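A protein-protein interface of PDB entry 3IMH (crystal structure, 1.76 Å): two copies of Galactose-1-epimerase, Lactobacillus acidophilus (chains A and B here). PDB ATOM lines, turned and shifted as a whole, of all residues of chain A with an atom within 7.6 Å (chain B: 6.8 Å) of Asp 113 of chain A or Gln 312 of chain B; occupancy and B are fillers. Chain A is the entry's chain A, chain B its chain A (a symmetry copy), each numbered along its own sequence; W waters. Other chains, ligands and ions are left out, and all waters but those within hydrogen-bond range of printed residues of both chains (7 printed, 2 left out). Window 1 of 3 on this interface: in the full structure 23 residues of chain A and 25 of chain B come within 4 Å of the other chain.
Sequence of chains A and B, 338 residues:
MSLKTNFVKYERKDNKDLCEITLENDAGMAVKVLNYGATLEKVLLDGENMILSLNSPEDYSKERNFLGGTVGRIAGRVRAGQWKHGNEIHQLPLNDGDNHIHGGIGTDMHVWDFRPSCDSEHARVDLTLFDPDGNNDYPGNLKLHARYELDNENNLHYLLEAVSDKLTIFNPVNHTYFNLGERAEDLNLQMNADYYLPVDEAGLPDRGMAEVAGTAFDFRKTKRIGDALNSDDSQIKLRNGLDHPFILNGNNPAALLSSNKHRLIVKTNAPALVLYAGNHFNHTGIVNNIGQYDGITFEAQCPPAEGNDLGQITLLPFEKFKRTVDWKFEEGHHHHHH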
ATOM      1  N   LYS A  16      22.381 -16.313  32.524  1.00  0.00           N
ATOM      2  CA  LYS A  16      23.428 -16.554  31.528  1.00  0.00           C
ATOM      3  C   LYS A  16      24.475 -17.482  32.111  1.00  0.00           C
ATOM      4  O   LYS A  16      24.607 -17.608  33.334  1.00  0.00           O
ATOM      5  CB  LYS A  16      24.088 -15.242  31.080  1.00  0.00           C
ATOM      6  CG  LYS A  16      23.143 -14.315  30.335  1.00  0.00           C
ATOM      7  CD  LYS A  16      23.733 -12.959  30.052  1.00  0.00           C
ATOM      8  CE  LYS A  16      24.377 -12.943  28.690  1.00  0.00           C
ATOM      9  NZ  LYS A  16      23.834 -11.817  27.891  1.00  0.00           N
ATOM     10  N   ASP A  17      25.230 -18.129  31.233  1.00  0.00           N
ATOM     11  CA  ASP A  17      26.300 -19.013  31.690  1.00  0.00           C
ATOM     12  C   ASP A  17      27.577 -18.235  31.965  1.00  0.00           C
ATOM     13  O   ASP A  17      27.983 -17.367  31.165  1.00  0.00           O
ATOM     14  CB  ASP A  17      26.615 -20.063  30.625  1.00  0.00           C
ATOM     15  CG  ASP A  17      25.450 -20.984  30.346  1.00  0.00           C
ATOM     16  OD1 ASP A  17      24.677 -21.291  31.269  1.00  0.00           O
ATOM     17  OD2 ASP A  17      25.324 -21.403  29.186  1.00  0.00           O
ATOM     18  N   ILE A  21      37.464 -19.169  29.864  1.00  0.00           N
ATOM     19  CA  ILE A  21      37.988 -19.398  28.515  1.00  0.00           C
ATOM     20  C   ILE A  21      39.507 -19.479  28.613  1.00  0.00           C
ATOM     21  O   ILE A  21      40.117 -18.632  29.256  1.00  0.00           O
ATOM     22  CB  ILE A  21      37.600 -18.235  27.547  1.00  0.00           C
ATOM     23  CG1 ILE A  21      36.076 -18.104  27.421  1.00  0.00           C
ATOM     24  CG2 ILE A  21      38.222 -18.426  26.165  1.00  0.00           C
ATOM     25  CD1 ILE A  21      35.546 -16.848  28.077  1.00  0.00           C
ATOM     26  N   ASN A  35      34.011 -14.614  31.009  1.00  0.00           N
ATOM     27  CA  ASN A  35      33.044 -13.706  30.377  1.00  0.00           C
ATOM     28  C   ASN A  35      32.318 -12.801  31.394  1.00  0.00           C
ATOM     29  O   ASN A  35      31.873 -11.711  31.036  1.00  0.00           O
ATOM     30  CB  ASN A  35      32.078 -14.412  29.421  1.00  0.00           C
ATOM     31  CG  ASN A  35      31.222 -15.450  30.116  1.00  0.00           C
ATOM     32  OD1 ASN A  35      31.735 -16.334  30.808  1.00  0.00           O
ATOM     33  ND2 ASN A  35      29.910 -15.348  29.943  1.00  0.00           N
ATOM     34  N   TYR A  36      32.276 -13.224  32.660  1.00  0.00           N
ATOM     35  CA  TYR A  36      31.871 -12.331  33.741  1.00  0.00           C
ATOM     36  C   TYR A  36      32.852 -11.139  33.793  1.00  0.00           C
ATOM     37  O   TYR A  36      34.048 -11.318  34.049  1.00  0.00           O
ATOM     38  CB  TYR A  36      31.847 -13.049  35.108  1.00  0.00           C
ATOM     39  CG  TYR A  36      31.532 -12.081  36.222  1.00  0.00           C
ATOM     40  CD1 TYR A  36      30.217 -11.695  36.463  1.00  0.00           C
ATOM     41  CD2 TYR A  36      32.551 -11.526  37.018  1.00  0.00           C
ATOM     42  CE1 TYR A  36      29.906 -10.792  37.462  1.00  0.00           C
ATOM     43  CE2 TYR A  36      32.252 -10.604  38.031  1.00  0.00           C
ATOM     44  CZ  TYR A  36      30.927 -10.258  38.250  1.00  0.00           C
ATOM     45  OH  TYR A  36      30.596  -9.357  39.231  1.00  0.00           O
ATOM     46  N   ALA A  38      34.237  -9.512  31.432  1.00  0.00           N
ATOM     47  CA  ALA A  38      35.342  -9.610  30.449  1.00  0.00           C
ATOM     48  C   ALA A  38      36.676  -9.505  31.178  1.00  0.00           C
ATOM     49  O   ALA A  38      37.498  -8.611  30.926  1.00  0.00           O
ATOM     50  CB  ALA A  38      35.216  -8.529  29.356  1.00  0.00           C
ATOM     51  N   HIS A 110      28.929  -7.184  34.966  1.00  0.00           N
ATOM     52  CA  HIS A 110      27.973  -7.754  34.013  1.00  0.00           C
ATOM     53  C   HIS A 110      28.506  -9.000  33.320  1.00  0.00           C
ATOM     54  O   HIS A 110      29.720  -9.171  33.178  1.00  0.00           O
ATOM     55  CB  HIS A 110      27.585  -6.699  32.967  1.00  0.00           C
ATOM     56  CG  HIS A 110      26.725  -5.611  33.525  1.00  0.00           C
ATOM     57  ND1 HIS A 110      27.229  -4.587  34.296  1.00  0.00           N
ATOM     58  CD2 HIS A 110      25.388  -5.403  33.452  1.00  0.00           C
ATOM     59  CE1 HIS A 110      26.244  -3.786  34.660  1.00  0.00           C
ATOM     60  NE2 HIS A 110      25.117  -4.259  34.161  1.00  0.00           N
ATOM     61  N   VAL A 111      27.590  -9.871  32.887  1.00  0.00           N
ATOM     62  CA  VAL A 111      27.977 -11.063  32.136  1.00  0.00           C
ATOM     63  C   VAL A 111      28.016 -10.717  30.647  1.00  0.00           C
ATOM     64  O   VAL A 111      26.994 -10.340  30.053  1.00  0.00           O
ATOM     65  CB  VAL A 111      26.999 -12.246  32.356  1.00  0.00           C
ATOM     66  CG1 VAL A 111      27.561 -13.497  31.702  1.00  0.00           C
ATOM     67  CG2 VAL A 111      26.758 -12.475  33.859  1.00  0.00           C
ATOM     68  N   TRP A 112      29.193 -10.841  30.052  1.00  0.00           N
ATOM     69  CA  TRP A 112      29.377 -10.514  28.638  1.00  0.00           C
ATOM     70  C   TRP A 112      29.143 -11.791  27.828  1.00  0.00           C
ATOM     71  O   TRP A 112      29.330 -12.900  28.331  1.00  0.00           O
ATOM     72  CB  TRP A 112      30.804 -10.021  28.367  1.00  0.00           C
ATOM     73  CG  TRP A 112      31.211  -8.707  29.013  1.00  0.00           C
ATOM     74  CD1 TRP A 112      31.089  -8.348  30.343  1.00  0.00           C
ATOM     75  CD2 TRP A 112      31.878  -7.610  28.365  1.00  0.00           C
ATOM     76  NE1 TRP A 112      31.612  -7.082  30.542  1.00  0.00           N
ATOM     77  CE2 TRP A 112      32.098  -6.611  29.348  1.00  0.00           C
ATOM     78  CE3 TRP A 112      32.285  -7.365  27.034  1.00  0.00           C
ATOM     79  CZ2 TRP A 112      32.722  -5.384  29.054  1.00  0.00           C
ATOM     80  CZ3 TRP A 112      32.908  -6.140  26.739  1.00  0.00           C
ATOM     81  CH2 TRP A 112      33.124  -5.169  27.749  1.00  0.00           C
ATOM     82  N   ASP A 113      28.728 -11.637  26.576  1.00  0.00           N
ATOM     83  CA  ASP A 113      28.723 -12.769  25.652  1.00  0.00           C
ATOM     84  C   ASP A 113      30.136 -12.933  25.135  1.00  0.00           C
ATOM     85  O   ASP A 113      30.945 -12.006  25.262  1.00  0.00           O
ATOM     86  CB  ASP A 113      27.727 -12.530  24.525  1.00  0.00           C
ATOM     87  CG  ASP A 113      26.283 -12.620  25.021  1.00  0.00           C
ATOM     88  OD1 ASP A 113      25.832 -13.725  25.395  1.00  0.00           O
ATOM     89  OD2 ASP A 113      25.622 -11.583  25.070  1.00  0.00           O
ATOM     90  N   PHE A 114      30.463 -14.105  24.584  1.00  0.00           N
ATOM     91  CA  PHE A 114      31.834 -14.336  24.131  1.00  0.00           C
ATOM     92  C   PHE A 114      31.891 -15.304  22.956  1.00  0.00           C
ATOM     93  O   PHE A 114      30.951 -16.077  22.732  1.00  0.00           O
ATOM     94  CB  PHE A 114      32.732 -14.823  25.288  1.00  0.00           C
ATOM     95  CG  PHE A 114      32.470 -16.250  25.711  1.00  0.00           C
ATOM     96  CD1 PHE A 114      33.229 -17.305  25.169  1.00  0.00           C
ATOM     97  CD2 PHE A 114      31.466 -16.541  26.626  1.00  0.00           C
ATOM     98  CE1 PHE A 114      32.973 -18.637  25.546  1.00  0.00           C
ATOM     99  CE2 PHE A 114      31.210 -17.870  27.019  1.00  0.00           C
ATOM    100  CZ  PHE A 114      31.958 -18.911  26.471  1.00  0.00           C
ATOM    101  N   ARG A 115      33.023 -15.285  22.254  1.00  0.00           N
ATOM    102  CA  ARG A 115      33.264 -16.185  21.138  1.00  0.00           C
ATOM    103  C   ARG A 115      34.777 -16.380  21.004  1.00  0.00           C
ATOM    104  O   ARG A 115      35.506 -15.425  20.745  1.00  0.00           O
ATOM    105  CB  ARG A 115      32.673 -15.611  19.842  1.00  0.00           C
ATOM    106  CG  ARG A 115      32.950 -16.493  18.624  1.00  0.00           C
ATOM    107  CD  ARG A 115      32.376 -15.867  17.356  1.00  0.00           C
ATOM    108  NE  ARG A 115      33.107 -14.666  16.932  1.00  0.00           N
ATOM    109  CZ  ARG A 115      34.132 -14.677  16.090  1.00  0.00           C
ATOM    110  NH1 ARG A 115      34.576 -15.828  15.580  1.00  0.00           N
ATOM    111  NH2 ARG A 115      34.717 -13.528  15.755  1.00  0.00           N
ATOM    112  N   VAL A 125      39.777 -14.471  22.320  1.00  0.00           N
ATOM    113  CA  VAL A 125      38.375 -14.476  22.680  1.00  0.00           C
ATOM    114  C   VAL A 125      37.823 -13.057  22.532  1.00  0.00           C
ATOM    115  O   VAL A 125      38.429 -12.101  23.009  1.00  0.00           O
ATOM    116  CB  VAL A 125      38.121 -15.080  24.092  1.00  0.00           C
ATOM    117  CG1 VAL A 125      38.929 -14.346  25.204  1.00  0.00           C
ATOM    118  CG2 VAL A 125      36.607 -15.111  24.413  1.00  0.00           C
ATOM    119  N   ASP A 126      36.717 -12.946  21.798  1.00  0.00           N
ATOM    120  CA  ASP A 126      36.002 -11.681  21.600  1.00  0.00           C
ATOM    121  C   ASP A 126      34.817 -11.701  22.533  1.00  0.00           C
ATOM    122  O   ASP A 126      34.136 -12.720  22.632  1.00  0.00           O
ATOM    123  CB  ASP A 126      35.516 -11.564  20.152  1.00  0.00           C
ATOM    124  CG  ASP A 126      36.637 -11.206  19.190  1.00  0.00           C
ATOM    125  OD1 ASP A 126      37.147 -10.071  19.275  1.00  0.00           O
ATOM    126  OD2 ASP A 126      37.015 -12.052  18.358  1.00  0.00           O
ATOM    127  N   LEU A 127      34.596 -10.605  23.252  1.00  0.00           N
ATOM    128  CA  LEU A 127      33.466 -10.521  24.192  1.00  0.00           C
ATOM    129  C   LEU A 127      32.656  -9.296  23.851  1.00  0.00           C
ATOM    130  O   LEU A 127      33.208  -8.298  23.394  1.00  0.00           O
ATOM    131  CB  LEU A 127      33.934 -10.448  25.651  1.00  0.00           C
ATOM    132  CG  LEU A 127      34.838 -11.607  26.098  1.00  0.00           C
ATOM    133  CD1 LEU A 127      36.309 -11.181  26.091  1.00  0.00           C
ATOM    134  CD2 LEU A 127      34.431 -12.042  27.479  1.00  0.00           C
ATOM    135  N   THR A 128      31.340  -9.376  24.036  1.00  0.00           N
ATOM    136  CA  THR A 128      30.497  -8.231  23.735  1.00  0.00           C
ATOM    137  C   THR A 128      29.490  -8.011  24.849  1.00  0.00           C
ATOM    138  O   THR A 128      29.055  -8.967  25.526  1.00  0.00           O
ATOM    139  CB  THR A 128      29.752  -8.377  22.374  1.00  0.00           C
ATOM    140  OG1 THR A 128      28.968  -9.571  22.391  1.00  0.00           O
ATOM    141  CG2 THR A 128      30.731  -8.432  21.185  1.00  0.00           C
ATOM    142  N   LEU A 129      29.095  -6.747  25.007  1.00  0.00           N
ATOM    143  CA  LEU A 129      28.111  -6.360  25.995  1.00  0.00           C
ATOM    144  C   LEU A 129      27.287  -5.210  25.460  1.00  0.00           C
ATOM    145  O   LEU A 129      27.827  -4.273  24.874  1.00  0.00           O
ATOM    146  CB  LEU A 129      28.804  -5.935  27.301  1.00  0.00           C
ATOM    147  CG  LEU A 129      27.902  -5.499  28.473  1.00  0.00           C
ATOM    148  CD1 LEU A 129      27.052  -6.660  28.980  1.00  0.00           C
ATOM    149  CD2 LEU A 129      28.758  -4.931  29.610  1.00  0.00           C
ATOM    150  N   PHE A 130      25.975  -5.307  25.670  1.00  0.00           N
ATOM    151  CA  PHE A 130      25.067  -4.209  25.391  1.00  0.00           C
ATOM    152  C   PHE A 130      24.658  -3.574  26.707  1.00  0.00           C
ATOM    153  O   PHE A 130      24.179  -4.254  27.626  1.00  0.00           O
ATOM    154  CB  PHE A 130      23.812  -4.716  24.669  1.00  0.00           C
ATOM    155  CG  PHE A 130      22.760  -3.647  24.487  1.00  0.00           C
ATOM    156  CD1 PHE A 130      22.929  -2.683  23.507  1.00  0.00           C
ATOM    157  CD2 PHE A 130      21.632  -3.592  25.299  1.00  0.00           C
ATOM    158  CE1 PHE A 130      21.975  -1.674  23.317  1.00  0.00           C
ATOM    159  CE2 PHE A 130      20.670  -2.575  25.123  1.00  0.00           C
ATOM    160  CZ  PHE A 130      20.854  -1.620  24.124  1.00  0.00           C
ATOM    161  N   LYS A 143      27.331  -0.325  22.813  1.00  0.00           N
ATOM    162  CA  LYS A 143      27.801  -1.656  22.464  1.00  0.00           C
ATOM    163  C   LYS A 143      29.301  -1.697  22.718  1.00  0.00           C
ATOM    164  O   LYS A 143      30.019  -0.900  22.119  1.00  0.00           O
ATOM    165  CB  LYS A 143      27.541  -1.917  20.986  1.00  0.00           C
ATOM    166  CG  LYS A 143      27.375  -3.365  20.649  1.00  0.00           C
ATOM    167  CD  LYS A 143      25.951  -3.798  20.915  1.00  0.00           C
ATOM    168  CE  LYS A 143      25.690  -5.082  20.220  1.00  0.00           C
ATOM    169  NZ  LYS A 143      25.943  -4.977  18.757  1.00  0.00           N
ATOM    170  N   LEU A 144      29.743  -2.612  23.577  1.00  0.00           N
ATOM    171  CA  LEU A 144      31.158  -2.760  23.939  1.00  0.00           C
ATOM    172  C   LEU A 144      31.667  -4.052  23.354  1.00  0.00           C
ATOM    173  O   LEU A 144      30.941  -5.050  23.309  1.00  0.00           O
ATOM    174  CB  LEU A 144      31.337  -2.816  25.453  1.00  0.00           C
ATOM    175  CG  LEU A 144      30.960  -1.639  26.346  1.00  0.00           C
ATOM    176  CD1 LEU A 144      29.495  -1.716  26.754  1.00  0.00           C
ATOM    177  CD2 LEU A 144      31.854  -1.689  27.578  1.00  0.00           C
ATOM    178  N   ALA A 146      35.240  -6.358  23.686  1.00  0.00           N
ATOM    179  CA  ALA A 146      36.583  -6.565  24.256  1.00  0.00           C
ATOM    180  C   ALA A 146      37.194  -7.762  23.543  1.00  0.00           C
ATOM    181  O   ALA A 146      36.478  -8.706  23.212  1.00  0.00           O
ATOM    182  CB  ALA A 146      36.481  -6.841  25.772  1.00  0.00           C
ATOM    183  N   PHE B 170      18.639  -8.487  15.339  1.00  0.00           N
ATOM    184  CA  PHE B 170      18.897  -9.058  14.017  1.00  0.00           C
ATOM    185  C   PHE B 170      19.828 -10.260  14.160  1.00  0.00           C
ATOM    186  O   PHE B 170      20.926 -10.128  14.716  1.00  0.00           O
ATOM    187  CB  PHE B 170      19.547  -7.984  13.132  1.00  0.00           C
ATOM    188  CG  PHE B 170      19.722  -8.397  11.703  1.00  0.00           C
ATOM    189  CD1 PHE B 170      18.613  -8.604  10.877  1.00  0.00           C
ATOM    190  CD2 PHE B 170      20.994  -8.564  11.177  1.00  0.00           C
ATOM    191  CE1 PHE B 170      18.782  -8.994   9.535  1.00  0.00           C
ATOM    192  CE2 PHE B 170      21.172  -8.934   9.838  1.00  0.00           C
ATOM    193  CZ  PHE B 170      20.070  -9.149   9.023  1.00  0.00           C
ATOM    194  N   PRO B 271      29.216 -17.605  16.635  1.00  0.00           N
ATOM    195  CA  PRO B 271      29.605 -18.353  17.830  1.00  0.00           C
ATOM    196  C   PRO B 271      28.944 -19.734  17.949  1.00  0.00           C
ATOM    197  O   PRO B 271      29.354 -20.539  18.781  1.00  0.00           O
ATOM    198  CB  PRO B 271      29.147 -17.432  18.970  1.00  0.00           C
ATOM    199  CG  PRO B 271      27.895 -16.792  18.431  1.00  0.00           C
ATOM    200  CD  PRO B 271      28.198 -16.573  16.941  1.00  0.00           C
ATOM    201  N   CYS B 302      24.148 -16.366  16.077  1.00  0.00           N
ATOM    202  CA  CYS B 302      24.122 -16.319  17.536  1.00  0.00           C
ATOM    203  C   CYS B 302      23.008 -17.246  18.022  1.00  0.00           C
ATOM    204  O   CYS B 302      21.960 -17.354  17.368  1.00  0.00           O
ATOM    205  CB  CYS B 302      23.885 -14.900  18.043  1.00  0.00           C
ATOM    206  SG  CYS B 302      25.301 -13.835  17.643  1.00  0.00           S
ATOM    207  N   PRO B 303      23.236 -17.938  19.151  1.00  0.00           N
ATOM    208  CA  PRO B 303      22.233 -18.940  19.536  1.00  0.00           C
ATOM    209  C   PRO B 303      20.888 -18.332  19.961  1.00  0.00           C
ATOM    210  O   PRO B 303      20.850 -17.208  20.489  1.00  0.00           O
ATOM    211  CB  PRO B 303      22.889 -19.645  20.736  1.00  0.00           C
ATOM    212  CG  PRO B 303      23.865 -18.634  21.283  1.00  0.00           C
ATOM    213  CD  PRO B 303      24.380 -17.905  20.081  1.00  0.00           C
ATOM    214  N   ASP B 309      16.420 -11.212  27.087  1.00  0.00           N
ATOM    215  CA  ASP B 309      17.720 -10.560  27.006  1.00  0.00           C
ATOM    216  C   ASP B 309      18.365 -11.017  25.706  1.00  0.00           C
ATOM    217  O   ASP B 309      18.833 -12.156  25.599  1.00  0.00           O
ATOM    218  CB  ASP B 309      18.603 -10.899  28.216  1.00  0.00           C
ATOM    219  CG  ASP B 309      19.964 -10.206  28.181  1.00  0.00           C
ATOM    220  OD1 ASP B 309      20.354  -9.637  27.136  1.00  0.00           O
ATOM    221  OD2 ASP B 309      20.665 -10.240  29.210  1.00  0.00           O
ATOM    222  N   LEU B 310      18.366 -10.107  24.729  1.00  0.00           N
ATOM    223  CA  LEU B 310      18.888 -10.353  23.381  1.00  0.00           C
ATOM    224  C   LEU B 310      20.033  -9.388  23.058  1.00  0.00           C
ATOM    225  O   LEU B 310      20.214  -8.974  21.900  1.00  0.00           O
ATOM    226  CB  LEU B 310      17.757 -10.193  22.341  1.00  0.00           C
ATOM    227  CG  LEU B 310      16.466 -10.986  22.631  1.00  0.00           C
ATOM    228  CD1 LEU B 310      15.416 -10.661  21.586  1.00  0.00           C
ATOM    229  CD2 LEU B 310      16.761 -12.487  22.657  1.00  0.00           C
ATOM    230  N   GLY B 311      20.808  -9.036  24.086  1.00  0.00           N
ATOM    231  CA  GLY B 311      21.932  -8.101  23.923  1.00  0.00           C
ATOM    232  C   GLY B 311      22.884  -8.488  22.803  1.00  0.00           C
ATOM    233  O   GLY B 311      23.295  -7.629  22.019  1.00  0.00           O
ATOM    234  N   GLN B 312      23.197  -9.788  22.717  1.00  0.00           N
ATOM    235  CA  GLN B 312      24.145 -10.335  21.723  1.00  0.00           C
ATOM    236  C   GLN B 312      23.747  -9.989  20.273  1.00  0.00           C
ATOM    237  O   GLN B 312      24.606  -9.753  19.415  1.00  0.00           O
ATOM    238  CB  GLN B 312      24.257 -11.858  21.893  1.00  0.00           C
ATOM    239  CG  GLN B 312      25.391 -12.489  21.091  1.00  0.00           C
ATOM    240  CD  GLN B 312      25.646 -13.942  21.450  1.00  0.00           C
ATOM    241  OE1 GLN B 312      24.727 -14.687  21.786  1.00  0.00           O
ATOM    242  NE2 GLN B 312      26.904 -14.344  21.388  1.00  0.00           N
ATOM    243  N   ILE B 313      22.437  -9.933  20.027  1.00  0.00           N
ATOM    244  CA  ILE B 313      21.912  -9.684  18.673  1.00  0.00           C
ATOM    245  C   ILE B 313      21.327  -8.287  18.470  1.00  0.00           C
ATOM    246  O   ILE B 313      20.685  -8.011  17.448  1.00  0.00           O
ATOM    247  CB  ILE B 313      20.885 -10.774  18.241  1.00  0.00           C
ATOM    248  CG1 ILE B 313      19.604 -10.685  19.082  1.00  0.00           C
ATOM    249  CG2 ILE B 313      21.535 -12.164  18.339  1.00  0.00           C
ATOM    250  CD1 ILE B 313      18.399 -11.472  18.469  1.00  0.00           C
ATOM    251  N   THR B 314      21.568  -7.404  19.436  1.00  0.00           N
ATOM    252  CA  THR B 314      21.083  -6.034  19.358  1.00  0.00           C
ATOM    253  C   THR B 314      22.034  -5.241  18.468  1.00  0.00           C
ATOM    254  O   THR B 314      23.241  -5.390  18.566  1.00  0.00           O
ATOM    255  CB  THR B 314      20.979  -5.425  20.775  1.00  0.00           C
ATOM    256  OG1 THR B 314      20.028  -6.184  21.536  1.00  0.00           O
ATOM    257  CG2 THR B 314      20.520  -3.962  20.725  1.00  0.00           C
ATOM    258  N   LEU B 315      21.487  -4.423  17.583  1.00  0.00           N
ATOM    259  CA  LEU B 315      22.286  -3.509  16.770  1.00  0.00           C
ATOM    260  C   LEU B 315      21.907  -2.074  17.113  1.00  0.00           C
ATOM    261  O   LEU B 315      20.718  -1.745  17.179  1.00  0.00           O
ATOM    262  CB  LEU B 315      21.996  -3.740  15.282  1.00  0.00           C
ATOM    263  CG  LEU B 315      22.393  -5.064  14.623  1.00  0.00           C
ATOM    264  CD1 LEU B 315      21.905  -5.056  13.170  1.00  0.00           C
ATOM    265  CD2 LEU B 315      23.907  -5.267  14.692  1.00  0.00           C
HETATM  266  O   HOH W   1      27.700 -17.224  22.235  1.00  0.00           O
HETATM  267  O   HOH W   2      27.442 -10.187  19.820  1.00  0.00           O
HETATM  268  O   HOH W   3      29.325 -14.409  21.042  1.00  0.00           O
HETATM  269  O   HOH W   4      27.373  -7.781  19.746  1.00  0.00           O
HETATM  270  O   HOH W   5      22.952  -9.555  27.131  1.00  0.00           O
HETATM  271  O   HOH W   6      24.579  -7.806  17.360  1.00  0.00           O
HETATM  272  O   HOH W   7      26.223  -9.117  24.234  1.00  0.00           O
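The side-chain carboxylate of Asp 309 of chain B is in salt-bridge range of the side-chain amino group of Lys 16 of chain A, at 3.8 Å.
The side-chain amino group of Lys 143 of chain A lies within hydrogen-bond range of the backbone carbonyl oxygen of Thr 314 of chain B, at 2.7 Å.
NZ of Lys 16 of chain A is in salt-bridge range of OD2 of Asp 113 of chain A (3.3 Å).
O of Thr 128 of chain A lies within hydrogen-bond range of N of Asp 113 of chain A.
The guanidinium group of Arg 115 of chain A is in salt-bridge range of the side-chain carboxylate of Asp 126 of chain A, 3.8 Å away.
OD1 of Asp 309 of chain B sits at hydrogen-bond distance from N of Gly 311 of chain B, at 3.1 Å.
The side-chain hydroxyl of Thr 314 of chain B lies within hydrogen-bond range of the backbone carbonyl oxygen of Leu 310 of chain B, 2.8 Å away.
Among the printed residues, merely in contact across the chains: Asp 113 of chain A with Gln 312 of chain B, Arg 115 of chain A with Pro 271 of chain B, Phe 130 of chain A with Gly 311 of chain B, Phe 130 of chain A with Thr 314 of chain B and Lys 143 of chain A with Gly 311 of chain B.
Of the printed residues of chain B, Lys 16 of chain A touches Asp 309 (3.8 Å).
Ala 38 of chain A touches none of the printed residues of chain B.
Of chain B, only Gln 312 comes within 4 Å of Asp 113 of chain A.
Of the printed residues of chain B, Phe 130 of chain A touches Gly 311 and Thr 314.
Of the printed residues of chain B, Lys 143 of chain A touches Gly 311 and Thr 314.
Gln 312 of chain B touches one residue of chain A.
Of the printed residues of chain A, Thr 314 of chain B touches Phe 130 (3.8 Å) and Lys 143 (2.7 Å).
Of the 21 printed residues of chain A, 5 touch a printed residue of chain B.
Hydrophobic or aromatic side chains of chain A that line the printed part of chain B: Phe 130.
Hydrophobic or aromatic side chains of chain B that line the printed part of chain A: Pro 271.
Among the printed residues, Asp or Glu carboxylates within 4 Å of a Lys or Arg side-chain nitrogen of the other chain: Lys 16 of chain A with Asp 309 of chain B.
No position is printed for both chains.
Water W3 lies within hydrogen-bond range of NE2 of Gln 312 of chain B (2.4 Å) and O of Phe 114 of chain A (2.9 Å).
Water W5 bridges the side-chain amino group of Lys 16 of chain A (2.5 Å) and the side-chain carboxylate of Asp 309 of chain B (2.6 Å).
Water W6 lies within hydrogen-bond range of the backbone carbonyl oxygen (O) of Gln 312 of chain B, the backbone carbonyl oxygen (O) of Thr 314 of chain B and the side-chain amino group (NZ) of Lys 143 of chain A.
Water W2 bridges the backbone carbonyl oxygen of Gln 312 of chain B and the side-chain hydroxyl of Thr 128 of chain A.
Water W1 bridges NE2 of Gln 312 of chain B and O of Phe 114 of chain A.
Water W4 lies within hydrogen-bond range of NZ of Lys 143 of chain A and O of Gln 312 of chain B.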
